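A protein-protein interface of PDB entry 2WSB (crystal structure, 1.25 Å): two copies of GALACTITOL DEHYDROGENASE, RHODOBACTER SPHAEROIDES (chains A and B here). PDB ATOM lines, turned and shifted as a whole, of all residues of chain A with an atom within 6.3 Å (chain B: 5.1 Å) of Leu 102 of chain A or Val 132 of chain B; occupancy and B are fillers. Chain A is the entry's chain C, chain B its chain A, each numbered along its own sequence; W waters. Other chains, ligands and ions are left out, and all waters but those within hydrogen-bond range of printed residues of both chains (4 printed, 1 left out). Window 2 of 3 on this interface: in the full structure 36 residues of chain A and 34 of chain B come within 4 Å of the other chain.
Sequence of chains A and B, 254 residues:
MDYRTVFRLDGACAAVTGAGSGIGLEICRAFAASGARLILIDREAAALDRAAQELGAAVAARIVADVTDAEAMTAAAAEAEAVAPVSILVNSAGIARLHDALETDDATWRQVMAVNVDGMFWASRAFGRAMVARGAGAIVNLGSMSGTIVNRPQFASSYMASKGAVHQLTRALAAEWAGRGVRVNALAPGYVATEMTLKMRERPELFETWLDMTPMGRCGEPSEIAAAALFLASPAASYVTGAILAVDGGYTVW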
ATOM      1  N   ASP A 100     -24.760 -22.636  14.084  1.00  0.00           N
ATOM      2  CA  ASP A 100     -24.305 -21.382  14.713  1.00  0.00           C
ATOM      3  C   ASP A 100     -23.446 -20.576  13.727  1.00  0.00           C
ATOM      4  O   ASP A 100     -22.621 -21.191  12.997  1.00  0.00           O
ATOM      5  CB  ASP A 100     -23.495 -21.683  15.945  1.00  0.00           C
ATOM      6  CG  ASP A 100     -24.355 -22.312  17.063  1.00  0.00           C
ATOM      7  OD1 ASP A 100     -25.605 -22.546  16.905  1.00  0.00           O
ATOM      8  OD2 ASP A 100     -23.866 -22.519  18.212  1.00  0.00           O
ATOM      9  N   ALA A 101     -23.590 -19.245  13.728  1.00  0.00           N
ATOM     10  CA  ALA A 101     -22.917 -18.443  12.686  1.00  0.00           C
ATOM     11  C   ALA A 101     -21.443 -18.677  12.652  1.00  0.00           C
ATOM     12  O   ALA A 101     -20.851 -18.874  11.572  1.00  0.00           O
ATOM     13  CB  ALA A 101     -23.238 -16.961  13.029  1.00  0.00           C
ATOM     14  N   LEU A 102     -20.760 -18.734  13.806  1.00  0.00           N
ATOM     15  CA  LEU A 102     -19.317 -18.904  13.792  1.00  0.00           C
ATOM     16  C   LEU A 102     -18.832 -20.326  13.527  1.00  0.00           C
ATOM     17  O   LEU A 102     -17.638 -20.587  13.356  1.00  0.00           O
ATOM     18  CB  LEU A 102     -18.682 -18.405  15.065  1.00  0.00           C
ATOM     19  CG  LEU A 102     -18.839 -16.880  15.304  1.00  0.00           C
ATOM     20  CD1 LEU A 102     -18.401 -16.455  16.692  1.00  0.00           C
ATOM     21  CD2 LEU A 102     -18.195 -16.067  14.215  1.00  0.00           C
ATOM     22  N   GLU A 103     -19.750 -21.253  13.433  1.00  0.00           N
ATOM     23  CA  GLU A 103     -19.384 -22.636  13.066  1.00  0.00           C
ATOM     24  C   GLU A 103     -19.953 -23.000  11.692  1.00  0.00           C
ATOM     25  O   GLU A 103     -20.051 -24.163  11.295  1.00  0.00           O
ATOM     26  CB  GLU A 103     -19.903 -23.670  14.074  1.00  0.00           C
ATOM     27  CG  GLU A 103     -18.892 -23.792  15.119  1.00  0.00           C
ATOM     28  CD  GLU A 103     -19.168 -22.792  16.162  1.00  0.00           C
ATOM     29  OE1 GLU A 103     -18.235 -22.061  16.522  1.00  0.00           O
ATOM     30  OE2 GLU A 103     -20.315 -22.889  16.694  1.00  0.00           O
ATOM     31  N   THR A 104     -20.424 -22.065  10.963  1.00  0.00           N
ATOM     32  CA  THR A 104     -21.095 -22.288   9.704  1.00  0.00           C
ATOM     33  C   THR A 104     -20.124 -22.683   8.630  1.00  0.00           C
ATOM     34  O   THR A 104     -19.195 -21.959   8.344  1.00  0.00           O
ATOM     35  CB  THR A 104     -21.903 -21.055   9.226  1.00  0.00           C
ATOM     36  OG1 THR A 104     -22.849 -20.732  10.255  1.00  0.00           O
ATOM     37  CG2 THR A 104     -22.668 -21.321   7.949  1.00  0.00           C
ATOM     38  N   ARG B 125     -19.071 -13.221   9.514  1.00  0.00           N
ATOM     39  CA  ARG B 125     -18.506 -14.388  10.246  1.00  0.00           C
ATOM     40  C   ARG B 125     -16.979 -14.156  10.509  1.00  0.00           C
ATOM     41  O   ARG B 125     -16.504 -14.360  11.629  1.00  0.00           O
ATOM     42  CB  ARG B 125     -18.739 -15.627   9.384  1.00  0.00           C
ATOM     43  CG  ARG B 125     -18.233 -16.952  10.049  1.00  0.00           C
ATOM     44  CD  ARG B 125     -18.455 -18.168   9.166  1.00  0.00           C
ATOM     45  NE  ARG B 125     -17.544 -18.006   7.995  1.00  0.00           N
ATOM     46  CZ  ARG B 125     -17.645 -18.729   6.878  1.00  0.00           C
ATOM     47  NH1 ARG B 125     -18.568 -19.743   6.798  1.00  0.00           N
ATOM     48  NH2 ARG B 125     -16.839 -18.457   5.830  1.00  0.00           N
ATOM     49  N   GLY B 128     -16.576 -10.944  12.797  1.00  0.00           N
ATOM     50  CA  GLY B 128     -17.367 -11.093  14.032  1.00  0.00           C
ATOM     51  C   GLY B 128     -16.742 -12.105  14.994  1.00  0.00           C
ATOM     52  O   GLY B 128     -16.947 -11.982  16.199  1.00  0.00           O
ATOM     53  N   ARG B 129     -15.938 -13.057  14.511  1.00  0.00           N
ATOM     54  CA  ARG B 129     -15.339 -14.046  15.377  1.00  0.00           C
ATOM     55  C   ARG B 129     -14.558 -13.413  16.567  1.00  0.00           C
ATOM     56  O   ARG B 129     -14.847 -13.747  17.749  1.00  0.00           O
ATOM     57  CB  ARG B 129     -14.440 -14.996  14.549  1.00  0.00           C
ATOM     58  CG  ARG B 129     -14.022 -16.201  15.391  1.00  0.00           C
ATOM     59  CD  ARG B 129     -13.147 -17.173  14.532  1.00  0.00           C
ATOM     60  NE  ARG B 129     -13.895 -17.625  13.291  1.00  0.00           N
ATOM     61  CZ  ARG B 129     -14.891 -18.511  13.247  1.00  0.00           C
ATOM     62  NH1 ARG B 129     -15.187 -19.257  14.334  1.00  0.00           N
ATOM     63  NH2 ARG B 129     -15.478 -18.772  12.060  1.00  0.00           N
ATOM     64  N   ALA B 130     -13.633 -12.496  16.262  1.00  0.00           N
ATOM     65  CA  ALA B 130     -12.849 -11.896  17.307  1.00  0.00           C
ATOM     66  C   ALA B 130     -13.705 -10.929  18.138  1.00  0.00           C
ATOM     67  O   ALA B 130     -13.379 -10.749  19.342  1.00  0.00           O
ATOM     68  CB  ALA B 130     -11.595 -11.216  16.780  1.00  0.00           C
ATOM     69  N   MET B 131     -14.709 -10.274  17.537  1.00  0.00           N
ATOM     70  CA  MET B 131     -15.602  -9.394  18.311  1.00  0.00           C
ATOM     71  C   MET B 131     -16.309 -10.265  19.378  1.00  0.00           C
ATOM     72  O   MET B 131     -16.429  -9.872  20.560  1.00  0.00           O
ATOM     73  CB  MET B 131     -16.647  -8.716  17.413  1.00  0.00           C
ATOM     74  CG  MET B 131     -15.996  -7.801  16.436  1.00  0.00           C
ATOM     75  SD  MET B 131     -17.376  -7.133  15.442  1.00  0.00           S
ATOM     76  CE  MET B 131     -16.424  -6.204  14.172  1.00  0.00           C
ATOM     77  N   VAL B 132     -16.909 -11.396  18.957  1.00  0.00           N
ATOM     78  CA  VAL B 132     -17.572 -12.276  19.887  1.00  0.00           C
ATOM     79  C   VAL B 132     -16.649 -12.772  21.028  1.00  0.00           C
ATOM     80  O   VAL B 132     -17.003 -12.730  22.196  1.00  0.00           O
ATOM     81  CB  VAL B 132     -18.282 -13.461  19.149  1.00  0.00           C
ATOM     82  CG1 VAL B 132     -18.942 -14.483  20.079  1.00  0.00           C
ATOM     83  CG2 VAL B 132     -19.402 -12.872  18.224  1.00  0.00           C
ATOM     84  N   ALA B 133     -15.388 -13.032  20.643  1.00  0.00           N
ATOM     85  CA  ALA B 133     -14.443 -13.524  21.644  1.00  0.00           C
ATOM     86  C   ALA B 133     -14.129 -12.384  22.654  1.00  0.00           C
ATOM     87  O   ALA B 133     -13.942 -12.650  23.876  1.00  0.00           O
ATOM     88  CB  ALA B 133     -13.166 -14.080  20.966  1.00  0.00           C
ATOM     89  N   ARG B 134     -14.089 -11.118  22.252  1.00  0.00           N
ATOM     90  CA  ARG B 134     -13.841  -9.923  23.100  1.00  0.00           C
ATOM     91  C   ARG B 134     -15.099  -9.525  23.841  1.00  0.00           C
ATOM     92  O   ARG B 134     -15.008  -8.702  24.760  1.00  0.00           O
ATOM     93  CB  ARG B 134     -13.316  -8.681  22.275  1.00  0.00           C
ATOM     94  CG  ARG B 134     -11.800  -8.762  21.991  1.00  0.00           C
ATOM     95  CD  ARG B 134     -11.387  -7.531  21.307  1.00  0.00           C
ATOM     96  NE  ARG B 134     -11.919  -7.450  19.913  1.00  0.00           N
ATOM     97  CZ  ARG B 134     -11.308  -7.931  18.840  1.00  0.00           C
ATOM     98  NH1 ARG B 134     -10.132  -8.612  18.945  1.00  0.00           N
ATOM     99  NH2 ARG B 134     -11.869  -7.723  17.653  1.00  0.00           N
ATOM    100  N   GLY B 135     -16.253 -10.095  23.469  1.00  0.00           N
ATOM    101  CA  GLY B 135     -17.550  -9.710  24.048  1.00  0.00           C
ATOM    102  C   GLY B 135     -17.947  -8.287  23.614  1.00  0.00           C
ATOM    103  O   GLY B 135     -18.647  -7.616  24.428  1.00  0.00           O
ATOM    104  N   ALA B 136     -17.521  -7.802  22.480  1.00  0.00           N
ATOM    105  CA  ALA B 136     -17.877  -6.378  22.148  1.00  0.00           C
ATOM    106  C   ALA B 136     -17.687  -6.239  20.646  1.00  0.00           C
ATOM    107  O   ALA B 136     -16.727  -6.684  20.038  1.00  0.00           O
ATOM    108  CB  ALA B 136     -16.924  -5.445  22.859  1.00  0.00           C
ATOM    109  N   GLU B 176     -28.383 -13.620  17.594  1.00  0.00           N
ATOM    110  CA  GLU B 176     -27.475 -14.730  18.041  1.00  0.00           C
ATOM    111  C   GLU B 176     -26.332 -14.129  18.836  1.00  0.00           C
ATOM    112  O   GLU B 176     -25.808 -14.795  19.693  1.00  0.00           O
ATOM    113  CB  GLU B 176     -26.959 -15.436  16.766  1.00  0.00           C
ATOM    114  CG  GLU B 176     -26.010 -16.558  17.048  1.00  0.00           C
ATOM    115  CD  GLU B 176     -25.751 -17.443  15.886  1.00  0.00           C
ATOM    116  OE1 GLU B 176     -26.354 -17.296  14.780  1.00  0.00           O
ATOM    117  OE2 GLU B 176     -24.836 -18.338  15.995  1.00  0.00           O
ATOM    118  N   TRP B 177     -25.872 -12.883  18.565  1.00  0.00           N
ATOM    119  CA  TRP B 177     -24.661 -12.338  19.236  1.00  0.00           C
ATOM    120  C   TRP B 177     -25.046 -11.330  20.352  1.00  0.00           C
ATOM    121  O   TRP B 177     -24.151 -10.764  20.964  1.00  0.00           O
ATOM    122  CB  TRP B 177     -23.702 -11.738  18.195  1.00  0.00           C
ATOM    123  CG  TRP B 177     -23.085 -12.800  17.341  1.00  0.00           C
ATOM    124  CD1 TRP B 177     -22.959 -14.146  17.540  1.00  0.00           C
ATOM    125  CD2 TRP B 177     -22.435 -12.548  16.094  1.00  0.00           C
ATOM    126  NE1 TRP B 177     -22.303 -14.764  16.509  1.00  0.00           N
ATOM    127  CE2 TRP B 177     -21.992 -13.802  15.598  1.00  0.00           C
ATOM    128  CE3 TRP B 177     -22.237 -11.371  15.295  1.00  0.00           C
ATOM    129  CZ2 TRP B 177     -21.301 -13.941  14.385  1.00  0.00           C
ATOM    130  CZ3 TRP B 177     -21.559 -11.509  14.090  1.00  0.00           C
ATOM    131  CH2 TRP B 177     -21.058 -12.797  13.693  1.00  0.00           C
ATOM    132  N   ARG B 180     -23.602 -11.876  23.680  1.00  0.00           N
ATOM    133  CA  ARG B 180     -22.144 -11.753  23.692  1.00  0.00           C
ATOM    134  C   ARG B 180     -21.632 -10.388  23.280  1.00  0.00           C
ATOM    135  O   ARG B 180     -20.468 -10.247  22.985  1.00  0.00           O
ATOM    136  CB  ARG B 180     -21.515 -12.904  22.870  1.00  0.00           C
ATOM    137  CG  ARG B 180     -21.731 -14.208  23.601  1.00  0.00           C
ATOM    138  CD  ARG B 180     -21.368 -15.442  22.715  1.00  0.00           C
ATOM    139  NE  ARG B 180     -22.525 -15.624  21.821  1.00  0.00           N
ATOM    140  CZ  ARG B 180     -22.521 -16.535  20.825  1.00  0.00           C
ATOM    141  NH1 ARG B 180     -21.412 -17.332  20.691  1.00  0.00           N
ATOM    142  NH2 ARG B 180     -23.630 -16.767  20.057  1.00  0.00           N
ATOM    143  N   VAL B 182     -22.184  -8.090  20.833  1.00  0.00           N
ATOM    144  CA  VAL B 182     -21.973  -7.541  19.466  1.00  0.00           C
ATOM    145  C   VAL B 182     -23.330  -7.077  18.951  1.00  0.00           C
ATOM    146  O   VAL B 182     -24.220  -7.883  18.744  1.00  0.00           O
ATOM    147  CB  VAL B 182     -21.357  -8.613  18.535  1.00  0.00           C
ATOM    148  CG1 VAL B 182     -21.085  -7.992  17.127  1.00  0.00           C
ATOM    149  CG2 VAL B 182     -20.016  -9.135  19.175  1.00  0.00           C
HETATM  150  O   HOH W   1     -16.810 -21.360  10.409  1.00  0.00           O
HETATM  151  O   HOH W   2     -26.598 -18.864  12.467  1.00  0.00           O
HETATM  152  O   HOH W   3     -24.025 -19.127  18.528  1.00  0.00           O
HETATM  153  O   HOH W   4     -15.713 -22.229  15.510  1.00  0.00           O
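No position is printed for both chains. Of the 9 pairs that touch across the chains among the printed residues, none has its exchanged pair printed and touching as well.
Of the printed residues of chain B, Leu 102 of chain A touches Arg 125, Arg 129, Val 132 and Trp 177. Val 132 of chain B touches one residue of chain A. Of the printed residues of chain A, Arg 129 of chain B touches Leu 102 (3.0 Å). Of the printed residues of chain A, Glu 176 of chain B touches Asp 100 (3.3 Å) and Ala 101 (2.7 Å). Of the printed residues of chain A, Trp 177 of chain B touches Ala 101 (3.8 Å) and Leu 102 (3.8 Å). Val 182 of chain B touches none of the printed residues of chain A. Ala 133 of chain B touches none of the printed residues of chain A. The nearest residue of chain B that does not touch Leu 102 of chain A is Gly 128 of chain B (4.3 Å).
The guanidinium group (NH2) of Arg 180 of chain B sits at hydrogen-bond distance from the backbone carbonyl oxygen (O) of Glu 176 of chain B, 3.0 Å away. The backbone NH (N) of Val 182 of chain B is in hydrogen-bond range of the backbone carbonyl oxygen (O) of Trp 177 of chain B. The backbone carbonyl oxygen (O) of Asp 100 of chain A lies within hydrogen-bond range of the side-chain hydroxyl (OG1) of Thr 104 of chain A, 2.8 Å away. The backbone carbonyl oxygen of Ala 101 of chain A sits at hydrogen-bond distance from the side-chain hydroxyl of Thr 104 of chain A (3.0 Å).
Water W4 lies within hydrogen-bond range of OE1 of Glu 103 of chain A (2.7 Å), NH1 of Arg 129 of chain B (3.2 Å) and O of Leu 102 of chain A (3.3 Å). Water W3 lies within hydrogen-bond range of OE2 of Glu 176 of chain B (2.8 Å), NH2 of Arg 180 of chain B (2.8 Å) and OD2 of Asp 100 of chain A (3.4 Å). Water W2 lies within hydrogen-bond range of OE1 of Glu 176 of chain B (2.8 Å) and N of Ala 101 of chain A (3.3 Å). Water W1 lies within hydrogen-bond range of the backbone carbonyl oxygen (O) of Leu 102 of chain A (3.2 Å), the backbone carbonyl oxygen (O) of Thr 104 of chain A (3.2 Å) and the guanidinium group (NH2) of Arg 129 of chain B (3.3 Å).
Among the printed residues, pairs that only touch across the chains: Asp 100 of chain A with Glu 176 of chain B (3.3 Å), Ala 101 of chain A with Arg 125 of chain B (3.5 Å), Ala 101 of chain A with Trp 177 of chain B (3.8 Å), Leu 102 of chain A with Arg 125 of chain B (3.5 Å), Leu 102 of chain A with Val 132 of chain B (3.9 Å) and Leu 102 of chain A with Trp 177 of chain B (3.8 Å).
Of the 14 printed residues of chain B, 5 touch a printed residue of chain A. Of the 5 printed residues of chain A, 4 touch a printed residue of chain B. Among the printed residues, no Asp or Glu carboxylate lies within 4 Å of a Lys or Arg side-chain nitrogen of the other chain.
The backbone carbonyl oxygen (O) of Thr 104 of chain A lies within hydrogen-bond range of the guanidinium group (NH1) of Arg 125 of chain B (2.8 Å). O of Leu 102 of chain A lies within hydrogen-bond range of NH1 of Arg 129 of chain B, at 3.0 Å. The backbone NH (N) of Ala 101 of chain A lies within hydrogen-bond range of the side-chain carboxylate (OE2) of Glu 176 of chain B (2.7 Å).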
